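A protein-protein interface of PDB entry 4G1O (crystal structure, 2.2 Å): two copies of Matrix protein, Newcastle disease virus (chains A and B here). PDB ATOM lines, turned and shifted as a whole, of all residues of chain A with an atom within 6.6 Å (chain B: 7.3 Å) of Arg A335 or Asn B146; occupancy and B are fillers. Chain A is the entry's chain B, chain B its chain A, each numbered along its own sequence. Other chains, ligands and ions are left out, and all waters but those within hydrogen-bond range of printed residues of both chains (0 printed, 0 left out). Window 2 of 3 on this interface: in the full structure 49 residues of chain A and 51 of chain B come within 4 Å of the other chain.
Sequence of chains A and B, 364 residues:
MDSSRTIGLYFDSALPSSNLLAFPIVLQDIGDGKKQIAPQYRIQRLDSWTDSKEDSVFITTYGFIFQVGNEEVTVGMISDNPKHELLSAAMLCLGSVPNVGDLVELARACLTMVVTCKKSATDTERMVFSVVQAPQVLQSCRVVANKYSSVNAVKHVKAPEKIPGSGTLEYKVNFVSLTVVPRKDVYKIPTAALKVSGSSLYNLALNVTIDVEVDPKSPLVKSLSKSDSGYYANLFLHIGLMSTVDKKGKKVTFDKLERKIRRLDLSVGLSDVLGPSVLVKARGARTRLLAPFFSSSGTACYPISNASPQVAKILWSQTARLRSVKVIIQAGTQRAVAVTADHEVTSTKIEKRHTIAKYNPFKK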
ATOM      1  N   ALA A 331      31.160 -31.238  36.849  1.00  0.00           N
ATOM      2  CA  ALA A 331      31.777 -30.101  36.147  1.00  0.00           C
ATOM      3  C   ALA A 331      31.082 -28.771  36.520  1.00  0.00           C
ATOM      4  O   ALA A 331      29.893 -28.768  36.859  1.00  0.00           O
ATOM      5  CB  ALA A 331      31.735 -30.327  34.652  1.00  0.00           C
ATOM      6  N   THR A 333      30.156 -26.117  34.760  1.00  0.00           N
ATOM      7  CA  THR A 333      29.146 -25.557  33.872  1.00  0.00           C
ATOM      8  C   THR A 333      28.335 -26.699  33.303  1.00  0.00           C
ATOM      9  O   THR A 333      28.861 -27.794  33.057  1.00  0.00           O
ATOM     10  CB  THR A 333      29.761 -24.879  32.652  1.00  0.00           C
ATOM     11  OG1 THR A 333      30.414 -25.904  31.917  1.00  0.00           O
ATOM     12  CG2 THR A 333      30.779 -23.785  33.047  1.00  0.00           C
ATOM     13  N   GLN A 334      27.071 -26.401  33.048  1.00  0.00           N
ATOM     14  CA  GLN A 334      26.152 -27.360  32.505  1.00  0.00           C
ATOM     15  C   GLN A 334      26.646 -27.950  31.194  1.00  0.00           C
ATOM     16  O   GLN A 334      26.482 -29.158  30.988  1.00  0.00           O
ATOM     17  CB  GLN A 334      24.772 -26.721  32.355  1.00  0.00           C
ATOM     18  CG  GLN A 334      24.156 -26.377  33.695  1.00  0.00           C
ATOM     19  CD  GLN A 334      23.857 -27.617  34.529  1.00  0.00           C
ATOM     20  OE1 GLN A 334      22.816 -28.237  34.383  1.00  0.00           O
ATOM     21  NE2 GLN A 334      24.771 -27.975  35.406  1.00  0.00           N
ATOM     22  N   ARG A 335      27.261 -27.139  30.317  1.00  0.00           N
ATOM     23  CA  ARG A 335      27.813 -27.711  29.075  1.00  0.00           C
ATOM     24  C   ARG A 335      28.797 -28.868  29.375  1.00  0.00           C
ATOM     25  O   ARG A 335      28.737 -29.967  28.797  1.00  0.00           O
ATOM     26  CB  ARG A 335      28.449 -26.623  28.182  1.00  0.00           C
ATOM     27  CG  ARG A 335      29.377 -27.154  27.086  1.00  0.00           C
ATOM     28  CD  ARG A 335      29.809 -26.083  26.090  1.00  0.00           C
ATOM     29  NE  ARG A 335      28.733 -25.795  25.142  1.00  0.00           N
ATOM     30  CZ  ARG A 335      28.030 -24.665  25.109  1.00  0.00           C
ATOM     31  NH1 ARG A 335      28.285 -23.683  25.969  1.00  0.00           N
ATOM     32  NH2 ARG A 335      27.069 -24.513  24.206  1.00  0.00           N
ATOM     33  N   ALA A 336      29.684 -28.627  30.317  1.00  0.00           N
ATOM     34  CA  ALA A 336      30.715 -29.595  30.631  1.00  0.00           C
ATOM     35  C   ALA A 336      30.157 -30.854  31.329  1.00  0.00           C
ATOM     36  O   ALA A 336      30.594 -31.985  31.093  1.00  0.00           O
ATOM     37  CB  ALA A 336      31.773 -28.917  31.467  1.00  0.00           C
ATOM     38  N   VAL A 337      29.161 -30.635  32.162  1.00  0.00           N
ATOM     39  CA  VAL A 337      28.512 -31.691  32.931  1.00  0.00           C
ATOM     40  C   VAL A 337      27.967 -32.799  32.027  1.00  0.00           C
ATOM     41  O   VAL A 337      28.044 -33.973  32.370  1.00  0.00           O
ATOM     42  CB  VAL A 337      27.377 -31.074  33.776  1.00  0.00           C
ATOM     43  CG1 VAL A 337      26.584 -32.139  34.526  1.00  0.00           C
ATOM     44  CG2 VAL A 337      27.952 -30.076  34.758  1.00  0.00           C
ATOM     45  N   ALA A 338      27.411 -32.388  30.885  1.00  0.00           N
ATOM     46  CA  ALA A 338      26.904 -33.265  29.843  1.00  0.00           C
ATOM     47  C   ALA A 338      27.874 -34.326  29.386  1.00  0.00           C
ATOM     48  O   ALA A 338      27.455 -35.465  29.133  1.00  0.00           O
ATOM     49  CB  ALA A 338      26.481 -32.436  28.630  1.00  0.00           C
ATOM     50  N   VAL A 339      29.146 -33.952  29.240  1.00  0.00           N
ATOM     51  CA  VAL A 339      30.127 -34.853  28.629  1.00  0.00           C
ATOM     52  C   VAL A 339      31.176 -35.357  29.607  1.00  0.00           C
ATOM     53  O   VAL A 339      32.143 -36.016  29.204  1.00  0.00           O
ATOM     54  CB  VAL A 339      30.856 -34.225  27.415  1.00  0.00           C
ATOM     55  CG1 VAL A 339      29.923 -34.139  26.202  1.00  0.00           C
ATOM     56  CG2 VAL A 339      31.499 -32.880  27.775  1.00  0.00           C
ATOM     57  N   THR A 340      30.995 -35.042  30.887  1.00  0.00           N
ATOM     58  CA  THR A 340      31.951 -35.460  31.905  1.00  0.00           C
ATOM     59  C   THR A 340      31.260 -36.224  33.058  1.00  0.00           C
ATOM     60  O   THR A 340      30.169 -35.857  33.520  1.00  0.00           O
ATOM     61  CB  THR A 340      32.815 -34.272  32.417  1.00  0.00           C
ATOM     62  OG1 THR A 340      31.974 -33.303  33.028  1.00  0.00           O
ATOM     63  CG2 THR A 340      33.579 -33.573  31.269  1.00  0.00           C
ATOM     64  N   VAL B 128      20.030 -32.935  32.507  1.00  0.00           N
ATOM     65  CA  VAL B 128      21.007 -32.650  31.466  1.00  0.00           C
ATOM     66  C   VAL B 128      20.946 -33.760  30.420  1.00  0.00           C
ATOM     67  O   VAL B 128      21.191 -34.926  30.750  1.00  0.00           O
ATOM     68  CB  VAL B 128      22.428 -32.502  32.050  1.00  0.00           C
ATOM     69  CG1 VAL B 128      23.433 -32.350  30.939  1.00  0.00           C
ATOM     70  CG2 VAL B 128      22.501 -31.276  32.958  1.00  0.00           C
ATOM     71  N   SER B 130      22.393 -35.257  26.832  1.00  0.00           N
ATOM     72  CA  SER B 130      23.516 -35.265  25.921  1.00  0.00           C
ATOM     73  C   SER B 130      23.101 -35.839  24.582  1.00  0.00           C
ATOM     74  O   SER B 130      22.639 -36.986  24.497  1.00  0.00           O
ATOM     75  CB  SER B 130      24.668 -36.098  26.491  1.00  0.00           C
ATOM     76  OG  SER B 130      25.581 -35.282  27.183  1.00  0.00           O
ATOM     77  N   VAL B 131      23.247 -35.024  23.540  1.00  0.00           N
ATOM     78  CA  VAL B 131      23.056 -35.464  22.182  1.00  0.00           C
ATOM     79  C   VAL B 131      24.368 -36.109  21.806  1.00  0.00           C
ATOM     80  O   VAL B 131      25.365 -35.432  21.513  1.00  0.00           O
ATOM     81  CB  VAL B 131      22.738 -34.308  21.236  1.00  0.00           C
ATOM     82  CG1 VAL B 131      22.632 -34.809  19.796  1.00  0.00           C
ATOM     83  CG2 VAL B 131      21.433 -33.658  21.652  1.00  0.00           C
ATOM     84  N   GLN B 139      21.220 -31.092  12.659  1.00  0.00           N
ATOM     85  CA  GLN B 139      22.411 -30.361  13.116  1.00  0.00           C
ATOM     86  C   GLN B 139      22.222 -28.830  13.198  1.00  0.00           C
ATOM     87  O   GLN B 139      22.907 -28.142  13.954  1.00  0.00           O
ATOM     88  CB  GLN B 139      23.632 -30.753  12.263  1.00  0.00           C
ATOM     89  CG  GLN B 139      23.883 -32.267  12.174  1.00  0.00           C
ATOM     90  CD  GLN B 139      24.379 -32.882  13.486  1.00  0.00           C
ATOM     91  OE1 GLN B 139      24.983 -32.191  14.318  1.00  0.00           O
ATOM     92  NE2 GLN B 139      24.124 -34.188  13.675  1.00  0.00           N
ATOM     93  N   SER B 140      21.270 -28.322  12.435  1.00  0.00           N
ATOM     94  CA  SER B 140      20.839 -26.924  12.467  1.00  0.00           C
ATOM     95  C   SER B 140      20.362 -26.396  13.854  1.00  0.00           C
ATOM     96  O   SER B 140      20.823 -25.343  14.313  1.00  0.00           O
ATOM     97  CB  SER B 140      19.764 -26.723  11.378  1.00  0.00           C
ATOM     98  OG  SER B 140      19.113 -25.463  11.472  1.00  0.00           O
ATOM     99  N   CYS B 141      19.481 -27.124  14.532  1.00  0.00           N
ATOM    100  CA  CYS B 141      18.768 -26.567  15.699  1.00  0.00           C
ATOM    101  C   CYS B 141      19.634 -26.330  16.934  1.00  0.00           C
ATOM    102  O   CYS B 141      20.659 -26.999  17.110  1.00  0.00           O
ATOM    103  CB  CYS B 141      17.587 -27.463  16.090  1.00  0.00           C
ATOM    104  SG  CYS B 141      18.105 -29.082  16.697  1.00  0.00           S
ATOM    105  N   ARG B 142      19.178 -25.397  17.785  1.00  0.00           N
ATOM    106  CA  ARG B 142      19.836 -25.005  19.043  1.00  0.00           C
ATOM    107  C   ARG B 142      20.442 -26.173  19.823  1.00  0.00           C
ATOM    108  O   ARG B 142      21.587 -26.096  20.209  1.00  0.00           O
ATOM    109  CB  ARG B 142      18.883 -24.183  19.950  1.00  0.00           C
ATOM    110  CG  ARG B 142      19.516 -23.610  21.238  1.00  0.00           C
ATOM    111  CD  ARG B 142      18.532 -22.828  22.136  1.00  0.00           C
ATOM    112  NE  ARG B 142      17.163 -23.336  22.010  1.00  0.00           N
ATOM    113  CZ  ARG B 142      16.638 -24.303  22.767  1.00  0.00           C
ATOM    114  NH1 ARG B 142      17.356 -24.860  23.734  1.00  0.00           N
ATOM    115  NH2 ARG B 142      15.391 -24.719  22.561  1.00  0.00           N
ATOM    116  N   VAL B 143      19.684 -27.252  20.021  1.00  0.00           N
ATOM    117  CA  VAL B 143      20.098 -28.311  20.922  1.00  0.00           C
ATOM    118  C   VAL B 143      21.177 -29.220  20.315  1.00  0.00           C
ATOM    119  O   VAL B 143      22.154 -29.530  20.977  1.00  0.00           O
ATOM    120  CB  VAL B 143      18.896 -29.115  21.450  1.00  0.00           C
ATOM    121  CG1 VAL B 143      19.347 -30.453  22.000  1.00  0.00           C
ATOM    122  CG2 VAL B 143      18.144 -28.326  22.522  1.00  0.00           C
ATOM    123  N   VAL B 144      21.023 -29.630  19.061  1.00  0.00           N
ATOM    124  CA  VAL B 144      22.017 -30.509  18.464  1.00  0.00           C
ATOM    125  C   VAL B 144      23.302 -29.770  18.156  1.00  0.00           C
ATOM    126  O   VAL B 144      24.362 -30.285  18.447  1.00  0.00           O
ATOM    127  CB  VAL B 144      21.478 -31.264  17.242  1.00  0.00           C
ATOM    128  CG1 VAL B 144      22.582 -32.116  16.596  1.00  0.00           C
ATOM    129  CG2 VAL B 144      20.286 -32.118  17.662  1.00  0.00           C
ATOM    130  N   ALA B 145      23.210 -28.555  17.608  1.00  0.00           N
ATOM    131  CA  ALA B 145      24.390 -27.675  17.478  1.00  0.00           C
ATOM    132  C   ALA B 145      25.155 -27.665  18.784  1.00  0.00           C
ATOM    133  O   ALA B 145      26.330 -27.985  18.814  1.00  0.00           O
ATOM    134  CB  ALA B 145      23.997 -26.247  17.085  1.00  0.00           C
ATOM    135  N   ASN B 146      24.488 -27.326  19.871  1.00  0.00           N
ATOM    136  CA  ASN B 146      25.165 -27.300  21.161  1.00  0.00           C
ATOM    137  C   ASN B 146      25.515 -28.667  21.725  1.00  0.00           C
ATOM    138  O   ASN B 146      26.427 -28.757  22.530  1.00  0.00           O
ATOM    139  CB  ASN B 146      24.351 -26.520  22.183  1.00  0.00           C
ATOM    140  CG  ASN B 146      24.144 -25.088  21.773  1.00  0.00           C
ATOM    141  OD1 ASN B 146      25.059 -24.437  21.255  1.00  0.00           O
ATOM    142  ND2 ASN B 146      22.931 -24.584  21.991  1.00  0.00           N
ATOM    143  N   LYS B 147      24.789 -29.715  21.308  1.00  0.00           N
ATOM    144  CA  LYS B 147      25.092 -31.139  21.637  1.00  0.00           C
ATOM    145  C   LYS B 147      24.544 -31.546  23.004  1.00  0.00           C
ATOM    146  O   LYS B 147      24.752 -32.696  23.452  1.00  0.00           O
ATOM    147  CB  LYS B 147      26.610 -31.458  21.617  1.00  0.00           C
ATOM    148  CG  LYS B 147      27.358 -31.203  20.319  1.00  0.00           C
ATOM    149  CD  LYS B 147      27.473 -32.475  19.479  1.00  0.00           C
ATOM    150  CE  LYS B 147      28.876 -32.667  18.888  1.00  0.00           C
ATOM    151  NZ  LYS B 147      29.384 -31.536  18.049  1.00  0.00           N
ATOM    152  N   TYR B 148      23.876 -30.596  23.665  1.00  0.00           N
ATOM    153  CA  TYR B 148      23.401 -30.780  25.023  1.00  0.00           C
ATOM    154  C   TYR B 148      22.220 -29.851  25.317  1.00  0.00           C
ATOM    155  O   TYR B 148      22.039 -28.845  24.649  1.00  0.00           O
ATOM    156  CB  TYR B 148      24.553 -30.528  26.018  1.00  0.00           C
ATOM    157  CG  TYR B 148      24.681 -29.100  26.496  1.00  0.00           C
ATOM    158  CD1 TYR B 148      25.390 -28.146  25.755  1.00  0.00           C
ATOM    159  CD2 TYR B 148      24.095 -28.701  27.697  1.00  0.00           C
ATOM    160  CE1 TYR B 148      25.497 -26.835  26.201  1.00  0.00           C
ATOM    161  CE2 TYR B 148      24.199 -27.402  28.148  1.00  0.00           C
ATOM    162  CZ  TYR B 148      24.891 -26.476  27.405  1.00  0.00           C
ATOM    163  OH  TYR B 148      24.961 -25.185  27.882  1.00  0.00           O
ATOM    164  N   SER B 149      21.405 -30.190  26.301  1.00  0.00           N
ATOM    165  CA  SER B 149      20.484 -29.189  26.845  1.00  0.00           C
ATOM    166  C   SER B 149      20.348 -29.435  28.341  1.00  0.00           C
ATOM    167  O   SER B 149      20.172 -30.580  28.780  1.00  0.00           O
ATOM    168  CB  SER B 149      19.122 -29.227  26.132  1.00  0.00           C
ATOM    169  OG  SER B 149      18.337 -28.114  26.478  1.00  0.00           O
ATOM    170  N   SER B 150      20.470 -28.370  29.122  1.00  0.00           N
ATOM    171  CA  SER B 150      20.244 -28.451  30.568  1.00  0.00           C
ATOM    172  C   SER B 150      18.954 -27.781  30.913  1.00  0.00           C
ATOM    173  O   SER B 150      18.827 -26.582  30.728  1.00  0.00           O
ATOM    174  CB  SER B 150      21.332 -27.722  31.361  1.00  0.00           C
ATOM    175  OG  SER B 150      20.922 -27.633  32.711  1.00  0.00           O
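O of Ala A338 is in hydrogen-bond range of OG of Ser B130 (2.7 Å).
The side-chain amide oxygen (OE1) of Gln A334 is in hydrogen-bond range of the side-chain hydroxyl (OG) of Ser B150, at 2.6 Å.
The backbone NH of Tyr B148 lies within hydrogen-bond range of the backbone carbonyl oxygen of Val B143 (3.4 Å).
O of Arg B142 is in hydrogen-bond range of ND2 of Asn B146.
Among the printed residues, pairs that only touch across the chains: Gln A334 with Val B128 (3.4 Å), Arg A335 with Tyr B148 (3.4 Å), Arg A335 with Asn B146 (3.6 Å), Ala A338 with Val B128 (3.8 Å), Ala A338 with Tyr B148 (3.8 Å) and Gln A334 with Tyr B148 (3.9 Å).
Of the printed residues of chain B, Arg A335 touches Asn B146 (3.6 Å) and Tyr B148 (3.4 Å).
Printed residues of chain B within 4 Å of Ala A338: Val B128 (3.8 Å), Ser B130 (2.7 Å) and Tyr B148 (3.8 Å).
Of the printed residues of chain A, Ser B150 touches Gln A334.
Of the printed residues of chain A, Tyr B148 touches Gln A334 (3.9 Å), Arg A335 (3.4 Å) and Ala A338 (3.8 Å).
Val A339 touches none of the printed residues of chain B.
The nearest residue of chain B that does not touch Arg A335 is Ser B150 (6.0 Å).
The nearest printed residue of chain A that does not touch Asn B146 is Ala A338 (7.1 Å).
The nearest printed residue of chain A that does not touch Ser B150 is Arg A335 (6.0 Å).
Hydrophobic or aromatic side chains of chain B within 4 Å of the printed part of chain A: Val B128 and Tyr B148.
Along chain B the printed residues that touch a printed residue of chain A span positions 128 to 150.
No position is printed for both chains.
Of the 8 pairs that touch across the chains among the printed residues, none has its exchanged pair printed and touching as well.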
